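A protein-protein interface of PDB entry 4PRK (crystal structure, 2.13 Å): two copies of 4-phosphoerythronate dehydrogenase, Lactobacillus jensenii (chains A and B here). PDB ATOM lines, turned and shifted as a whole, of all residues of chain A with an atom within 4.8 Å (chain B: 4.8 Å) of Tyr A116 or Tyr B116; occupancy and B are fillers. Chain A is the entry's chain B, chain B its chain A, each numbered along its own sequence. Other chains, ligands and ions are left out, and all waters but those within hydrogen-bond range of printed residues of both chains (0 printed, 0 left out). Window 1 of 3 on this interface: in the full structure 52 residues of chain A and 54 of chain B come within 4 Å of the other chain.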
ATOM      1  N   THR A 112       6.539   4.568  -1.900  1.00  0.00           N
ATOM      2  CA  THR A 112       5.293   5.168  -2.350  1.00  0.00           C
ATOM      3  C   THR A 112       5.052   6.519  -1.649  1.00  0.00           C
ATOM      4  O   THR A 112       4.672   7.552  -2.273  1.00  0.00           O
ATOM      5  CB  THR A 112       4.110   4.218  -2.070  1.00  0.00           C
ATOM      6  OG1 THR A 112       4.253   3.050  -2.879  1.00  0.00           O
ATOM      7  CG2 THR A 112       2.812   4.860  -2.383  1.00  0.00           C
ATOM      8  N   GLN A 113       5.232   6.525  -0.349  1.00  0.00           N
ATOM      9  CA  GLN A 113       5.030   7.786   0.350  1.00  0.00           C
ATOM     10  C   GLN A 113       6.026   8.837  -0.089  1.00  0.00           C
ATOM     11  O   GLN A 113       5.660  10.021  -0.294  1.00  0.00           O
ATOM     12  CB  GLN A 113       5.133   7.567   1.850  1.00  0.00           C
ATOM     13  CG  GLN A 113       3.924   6.801   2.375  1.00  0.00           C
ATOM     14  CD  GLN A 113       3.838   6.795   3.883  1.00  0.00           C
ATOM     15  OE1 GLN A 113       4.352   7.693   4.571  1.00  0.00           O
ATOM     16  NE2 GLN A 113       3.163   5.798   4.410  1.00  0.00           N
ATOM     17  N   ALA A 114       7.262   8.405  -0.291  1.00  0.00           N
ATOM     18  CA  ALA A 114       8.263   9.353  -0.757  1.00  0.00           C
ATOM     19  C   ALA A 114       7.932   9.977  -2.104  1.00  0.00           C
ATOM     20  O   ALA A 114       8.044  11.204  -2.259  1.00  0.00           O
ATOM     21  CB  ALA A 114       9.615   8.717  -0.773  1.00  0.00           C
ATOM     22  N   MET A 115       7.430   9.160  -3.031  1.00  0.00           N
ATOM     23  CA  MET A 115       7.104   9.617  -4.365  1.00  0.00           C
ATOM     24  C   MET A 115       5.954  10.581  -4.327  1.00  0.00           C
ATOM     25  O   MET A 115       5.992  11.604  -4.960  1.00  0.00           O
ATOM     26  CB  MET A 115       6.652   8.483  -5.288  1.00  0.00           C
ATOM     27  CG  MET A 115       7.460   7.225  -5.130  1.00  0.00           C
ATOM     28  SD  MET A 115       8.116   6.572  -6.646  1.00  0.00           S
ATOM     29  CE  MET A 115       9.333   7.962  -6.752  1.00  0.00           C
ATOM     30  N   TYR A 116       4.871  10.196  -3.672  1.00  0.00           N
ATOM     31  CA  TYR A 116       3.715  11.103  -3.587  1.00  0.00           C
ATOM     32  C   TYR A 116       4.167  12.490  -3.028  1.00  0.00           C
ATOM     33  O   TYR A 116       3.793  13.532  -3.549  1.00  0.00           O
ATOM     34  CB  TYR A 116       2.639  10.448  -2.719  1.00  0.00           C
ATOM     35  CG  TYR A 116       1.403  11.273  -2.425  1.00  0.00           C
ATOM     36  CD1 TYR A 116       1.414  12.209  -1.422  1.00  0.00           C
ATOM     37  CD2 TYR A 116       0.230  11.039  -3.088  1.00  0.00           C
ATOM     38  CE1 TYR A 116       0.296  12.934  -1.119  1.00  0.00           C
ATOM     39  CE2 TYR A 116      -0.917  11.766  -2.810  1.00  0.00           C
ATOM     40  CZ  TYR A 116      -0.871  12.711  -1.831  1.00  0.00           C
ATOM     41  OH  TYR A 116      -1.946  13.438  -1.517  1.00  0.00           O
ATOM     42  N   LEU A 117       4.956  12.478  -1.960  1.00  0.00           N
ATOM     43  CA  LEU A 117       5.407  13.714  -1.303  1.00  0.00           C
ATOM     44  C   LEU A 117       6.375  14.465  -2.189  1.00  0.00           C
ATOM     45  O   LEU A 117       6.349  15.665  -2.224  1.00  0.00           O
ATOM     46  CB  LEU A 117       6.030  13.421   0.094  1.00  0.00           C
ATOM     47  CG  LEU A 117       5.067  12.784   1.075  1.00  0.00           C
ATOM     48  CD1 LEU A 117       5.710  12.194   2.303  1.00  0.00           C
ATOM     49  CD2 LEU A 117       4.019  13.790   1.516  1.00  0.00           C
ATOM     50  N   ASN A 118       7.212  13.747  -2.948  1.00  0.00           N
ATOM     51  CA  ASN A 118       8.061  14.401  -3.947  1.00  0.00           C
ATOM     52  C   ASN A 118       7.223  15.157  -5.012  1.00  0.00           C
ATOM     53  O   ASN A 118       7.552  16.270  -5.413  1.00  0.00           O
ATOM     54  CB  ASN A 118       8.946  13.326  -4.650  1.00  0.00           C
ATOM     55  CG  ASN A 118       9.947  13.950  -5.593  1.00  0.00           C
ATOM     56  OD1 ASN A 118      10.628  14.869  -5.206  1.00  0.00           O
ATOM     57  ND2 ASN A 118      10.015  13.482  -6.826  1.00  0.00           N
ATOM     58  N   ARG A 119       6.161  14.521  -5.503  1.00  0.00           N
ATOM     59  CA  ARG A 119       5.324  15.119  -6.512  1.00  0.00           C
ATOM     60  C   ARG A 119       4.328  16.142  -5.920  1.00  0.00           C
ATOM     61  O   ARG A 119       3.576  16.799  -6.672  1.00  0.00           O
ATOM     62  CB  ARG A 119       4.561  14.028  -7.236  1.00  0.00           C
ATOM     63  CG  ARG A 119       5.382  13.021  -8.010  1.00  0.00           C
ATOM     64  CD  ARG A 119       6.444  13.599  -8.922  1.00  0.00           C
ATOM     65  NE  ARG A 119       5.837  14.437  -9.917  1.00  0.00           N
ATOM     66  CZ  ARG A 119       6.091  14.427 -11.212  1.00  0.00           C
ATOM     67  NH1 ARG A 119       6.957  13.588 -11.723  1.00  0.00           N
ATOM     68  NH2 ARG A 119       5.414  15.240 -12.007  1.00  0.00           N
ATOM     69  N   LYS A 120       4.257  16.209  -4.578  1.00  0.00           N
ATOM     70  CA  LYS A 120       3.466  17.237  -3.843  1.00  0.00           C
ATOM     71  C   LYS A 120       2.013  17.181  -4.137  1.00  0.00           C
ATOM     72  O   LYS A 120       1.312  18.204  -4.243  1.00  0.00           O
ATOM     73  CB  LYS A 120       4.031  18.620  -4.144  1.00  0.00           C
ATOM     74  CG  LYS A 120       5.482  18.708  -3.658  1.00  0.00           C
ATOM     75  CD  LYS A 120       6.157  19.923  -4.269  1.00  0.00           C
ATOM     76  CE  LYS A 120       7.444  20.306  -3.606  1.00  0.00           C
ATOM     77  NZ  LYS A 120       7.938  21.467  -4.416  1.00  0.00           N
ATOM     78  N   ILE A 121       1.537  15.966  -4.266  1.00  0.00           N
ATOM     79  CA  ILE A 121       0.206  15.770  -4.785  1.00  0.00           C
ATOM     80  C   ILE A 121      -0.763  16.303  -3.766  1.00  0.00           C
ATOM     81  O   ILE A 121      -1.765  16.873  -4.146  1.00  0.00           O
ATOM     82  CB  ILE A 121      -0.038  14.287  -5.161  1.00  0.00           C
ATOM     83  CG1 ILE A 121       0.829  13.973  -6.391  1.00  0.00           C
ATOM     84  CG2 ILE A 121      -1.525  14.003  -5.440  1.00  0.00           C
ATOM     85  CD1 ILE A 121       0.927  12.499  -6.732  1.00  0.00           C
ATOM     86  N   GLY A 122      -0.427  16.166  -2.485  1.00  0.00           N
ATOM     87  CA  GLY A 122      -1.253  16.645  -1.395  1.00  0.00           C
ATOM     88  C   GLY A 122      -1.324  18.138  -1.337  1.00  0.00           C
ATOM     89  O   GLY A 122      -2.365  18.709  -1.062  1.00  0.00           O
ATOM     90  N   ILE A 291       1.993  12.468   5.111  1.00  0.00           N
ATOM     91  CA  ILE A 291       1.157  11.248   5.073  1.00  0.00           C
ATOM     92  C   ILE A 291       1.333  10.577   6.429  1.00  0.00           C
ATOM     93  O   ILE A 291       2.464  10.474   6.937  1.00  0.00           O
ATOM     94  CB  ILE A 291       1.648  10.298   3.959  1.00  0.00           C
ATOM     95  CG1 ILE A 291       1.180  10.770   2.578  1.00  0.00           C
ATOM     96  CG2 ILE A 291       1.234   8.865   4.227  1.00  0.00           C
ATOM     97  CD1 ILE A 291       1.968  10.206   1.384  1.00  0.00           C
ATOM     98  N   THR B 112       3.787   7.012  -9.467  1.00  0.00           N
ATOM     99  CA  THR B 112       3.551   7.514  -8.121  1.00  0.00           C
ATOM    100  C   THR B 112       2.079   7.419  -7.761  1.00  0.00           C
ATOM    101  O   THR B 112       1.700   6.922  -6.669  1.00  0.00           O
ATOM    102  CB  THR B 112       3.973   9.004  -8.043  1.00  0.00           C
ATOM    103  OG1 THR B 112       5.374   9.092  -8.116  1.00  0.00           O
ATOM    104  CG2 THR B 112       3.554   9.639  -6.802  1.00  0.00           C
ATOM    105  N   GLN B 113       1.225   7.907  -8.657  1.00  0.00           N
ATOM    106  CA  GLN B 113      -0.224   7.858  -8.386  1.00  0.00           C
ATOM    107  C   GLN B 113      -0.734   6.428  -8.290  1.00  0.00           C
ATOM    108  O   GLN B 113      -1.460   6.094  -7.340  1.00  0.00           O
ATOM    109  CB  GLN B 113      -1.008   8.593  -9.459  1.00  0.00           C
ATOM    110  CG  GLN B 113      -0.919  10.085  -9.292  1.00  0.00           C
ATOM    111  CD  GLN B 113      -1.895  10.874 -10.186  1.00  0.00           C
ATOM    112  OE1 GLN B 113      -2.965  10.400 -10.542  1.00  0.00           O
ATOM    113  NE2 GLN B 113      -1.513  12.113 -10.529  1.00  0.00           N
ATOM    114  N   ALA B 114      -0.293   5.565  -9.207  1.00  0.00           N
ATOM    115  CA  ALA B 114      -0.649   4.147  -9.126  1.00  0.00           C
ATOM    116  C   ALA B 114      -0.227   3.481  -7.808  1.00  0.00           C
ATOM    117  O   ALA B 114      -0.999   2.687  -7.260  1.00  0.00           O
ATOM    118  CB  ALA B 114      -0.102   3.334 -10.283  1.00  0.00           C
ATOM    119  N   MET B 115       0.973   3.807  -7.309  1.00  0.00           N
ATOM    120  CA  MET B 115       1.458   3.147  -6.118  1.00  0.00           C
ATOM    121  C   MET B 115       0.675   3.643  -4.917  1.00  0.00           C
ATOM    122  O   MET B 115       0.238   2.853  -4.104  1.00  0.00           O
ATOM    123  CB  MET B 115       2.946   3.365  -5.867  1.00  0.00           C
ATOM    124  CG  MET B 115       3.759   3.337  -7.120  1.00  0.00           C
ATOM    125  SD  MET B 115       5.361   2.671  -6.814  1.00  0.00           S
ATOM    126  CE  MET B 115       4.560   1.021  -6.658  1.00  0.00           C
ATOM    127  N   TYR B 116       0.523   4.948  -4.799  1.00  0.00           N
ATOM    128  CA  TYR B 116      -0.323   5.497  -3.718  1.00  0.00           C
ATOM    129  C   TYR B 116      -1.716   4.856  -3.662  1.00  0.00           C
ATOM    130  O   TYR B 116      -2.171   4.387  -2.603  1.00  0.00           O
ATOM    131  CB  TYR B 116      -0.423   7.002  -3.830  1.00  0.00           C
ATOM    132  CG  TYR B 116      -1.283   7.674  -2.796  1.00  0.00           C
ATOM    133  CD1 TYR B 116      -2.617   7.732  -2.978  1.00  0.00           C
ATOM    134  CD2 TYR B 116      -0.731   8.350  -1.713  1.00  0.00           C
ATOM    135  CE1 TYR B 116      -3.447   8.347  -2.081  1.00  0.00           C
ATOM    136  CE2 TYR B 116      -1.532   9.021  -0.799  1.00  0.00           C
ATOM    137  CZ  TYR B 116      -2.900   8.988  -1.007  1.00  0.00           C
ATOM    138  OH  TYR B 116      -3.774   9.593  -0.231  1.00  0.00           O
ATOM    139  N   LEU B 117      -2.394   4.835  -4.794  1.00  0.00           N
ATOM    140  CA  LEU B 117      -3.719   4.224  -4.838  1.00  0.00           C
ATOM    141  C   LEU B 117      -3.689   2.760  -4.562  1.00  0.00           C
ATOM    142  O   LEU B 117      -4.584   2.287  -3.924  1.00  0.00           O
ATOM    143  CB  LEU B 117      -4.418   4.495  -6.161  1.00  0.00           C
ATOM    144  CG  LEU B 117      -4.642   5.970  -6.393  1.00  0.00           C
ATOM    145  CD1 LEU B 117      -5.117   6.259  -7.785  1.00  0.00           C
ATOM    146  CD2 LEU B 117      -5.617   6.499  -5.326  1.00  0.00           C
ATOM    147  N   ASN B 118      -2.647   2.054  -5.027  1.00  0.00           N
ATOM    148  CA  ASN B 118      -2.450   0.617  -4.732  1.00  0.00           C
ATOM    149  C   ASN B 118      -2.286   0.379  -3.278  1.00  0.00           C
ATOM    150  O   ASN B 118      -2.783  -0.589  -2.771  1.00  0.00           O
ATOM    151  CB  ASN B 118      -1.243   0.032  -5.468  1.00  0.00           C
ATOM    152  CG  ASN B 118      -0.965  -1.419  -5.110  1.00  0.00           C
ATOM    153  OD1 ASN B 118      -1.756  -2.313  -5.418  1.00  0.00           O
ATOM    154  ND2 ASN B 118       0.213  -1.677  -4.542  1.00  0.00           N
ATOM    155  N   ARG B 119      -1.593   1.275  -2.597  1.00  0.00           N
ATOM    156  CA  ARG B 119      -1.432   1.160  -1.158  1.00  0.00           C
ATOM    157  C   ARG B 119      -2.659   1.708  -0.368  1.00  0.00           C
ATOM    158  O   ARG B 119      -2.688   1.630   0.898  1.00  0.00           O
ATOM    159  CB  ARG B 119      -0.132   1.894  -0.738  1.00  0.00           C
ATOM    160  CG  ARG B 119       1.151   1.293  -1.342  1.00  0.00           C
ATOM    161  CD  ARG B 119       1.286  -0.228  -1.118  1.00  0.00           C
ATOM    162  NE  ARG B 119       1.232  -0.557   0.318  1.00  0.00           N
ATOM    163  CZ  ARG B 119       2.153  -1.237   1.034  1.00  0.00           C
ATOM    164  NH1 ARG B 119       3.258  -1.743   0.507  1.00  0.00           N
ATOM    165  NH2 ARG B 119       1.929  -1.468   2.323  1.00  0.00           N
ATOM    166  N   LYS B 120      -3.621   2.296  -1.096  1.00  0.00           N
ATOM    167  CA  LYS B 120      -4.884   2.815  -0.527  1.00  0.00           C
ATOM    168  C   LYS B 120      -4.672   3.778   0.607  1.00  0.00           C
ATOM    169  O   LYS B 120      -5.452   3.807   1.584  1.00  0.00           O
ATOM    170  CB  LYS B 120      -5.781   1.660  -0.062  1.00  0.00           C
ATOM    171  CG  LYS B 120      -5.922   0.570  -1.119  1.00  0.00           C
ATOM    172  CD  LYS B 120      -6.638  -0.665  -0.578  1.00  0.00           C
ATOM    173  CE  LYS B 120      -7.177  -1.485  -1.727  1.00  0.00           C
ATOM    174  NZ  LYS B 120      -7.683  -2.793  -1.262  1.00  0.00           N
ATOM    175  N   ILE B 121      -3.640   4.604   0.466  1.00  0.00           N
ATOM    176  CA  ILE B 121      -3.272   5.520   1.505  1.00  0.00           C
ATOM    177  C   ILE B 121      -4.428   6.486   1.790  1.00  0.00           C
ATOM    178  O   ILE B 121      -4.649   6.842   2.946  1.00  0.00           O
ATOM    179  CB  ILE B 121      -1.990   6.262   1.171  1.00  0.00           C
ATOM    180  CG1 ILE B 121      -0.796   5.274   1.161  1.00  0.00           C
ATOM    181  CG2 ILE B 121      -1.738   7.400   2.144  1.00  0.00           C
ATOM    182  CD1 ILE B 121       0.477   5.795   0.488  1.00  0.00           C
ATOM    183  N   GLY B 122      -5.143   6.907   0.755  1.00  0.00           N
ATOM    184  CA  GLY B 122      -6.208   7.867   0.897  1.00  0.00           C
ATOM    185  C   GLY B 122      -7.422   7.246   1.533  1.00  0.00           C
ATOM    186  O   GLY B 122      -8.142   7.902   2.253  1.00  0.00           O
ATOM    187  N   ILE B 291      -7.099  10.136  -7.133  1.00  0.00           N
ATOM    188  CA  ILE B 291      -6.253  11.305  -7.117  1.00  0.00           C
ATOM    189  C   ILE B 291      -6.585  12.146  -8.319  1.00  0.00           C
ATOM    190  O   ILE B 291      -6.723  11.601  -9.404  1.00  0.00           O
ATOM    191  CB  ILE B 291      -4.759  10.933  -7.184  1.00  0.00           C
ATOM    192  CG1 ILE B 291      -4.250  10.417  -5.863  1.00  0.00           C
ATOM    193  CG2 ILE B 291      -3.889  12.123  -7.537  1.00  0.00           C
ATOM    194  CD1 ILE B 291      -2.832   9.858  -5.972  1.00  0.00           C
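The backbone carbonyl oxygen (O) of Tyr B116 lies within hydrogen-bond range of the backbone NH (N) of Ile B121, at 3.4 Å.
The backbone NH (N) of Gly B122 is in hydrogen-bond range of the side-chain hydroxyl (OH) of Tyr B116.
The backbone NH of Ile A121 lies within hydrogen-bond range of the backbone carbonyl oxygen of Tyr A116 (3.4 Å).
The side-chain hydroxyl of Tyr A116 sits at hydrogen-bond distance from the backbone NH of Gly A122 (3.3 Å).
Among the printed residues, pairs that only touch across the chains: Thr A112 with Met B115, Thr A112 with Tyr B116, Thr A112 with Arg B119, Thr A112 with Ile B121, Met A115 with Thr B112, Tyr A116 with Thr B112, Tyr A116 with Tyr B116, Arg A119 with Thr B112, Ile A121 with Thr B112, Ile A121 with Gln B113, Ile A121 with Ile B291 and Ile A291 with Ile B121.
Tyr A116 touches just these residues of chain B: Thr B112 and Tyr B116.
Of the printed residues of chain B, Ile A121 touches Thr B112 (3.9 Å), Gln B113 (3.97 Å) and Ile B291 (3.7 Å).
Gly A122 touches none of the printed residues of chain B.
Of the printed residues of chain B, Ile A291 touches Ile B121.
Of the printed residues of chain A, Thr B112 touches Met A115, Tyr A116, Arg A119 and Ile A121.
Of chain A, only Thr A112 (3.3 Å) and Tyr A116 (3.2 Å) come within 4 Å of Tyr B116.
Printed residues of chain A within 4 Å of Arg B119: Thr A112 (3.9 Å).
The nearest residue of chain A that does not touch Tyr B116 is Ile A291 (4.3 Å).
Of the 12 printed residues of chain A, 6 touch a printed residue of chain B.
Among the printed residues, 12 pairs touch across the chains.
Thr A112 touches Arg B119, and with the chains exchanged Arg A119 touches Thr B112.
Thr A112 touches Ile B121, and with the chains exchanged Ile A121 touches Thr B112.
Ile A121 touches Gln B113, but with the chains exchanged Gln A113 does not touch Ile B121 (4.1 Å).
Ile A121 touches Ile B291, and with the chains exchanged Ile A291 touches Ile B121.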
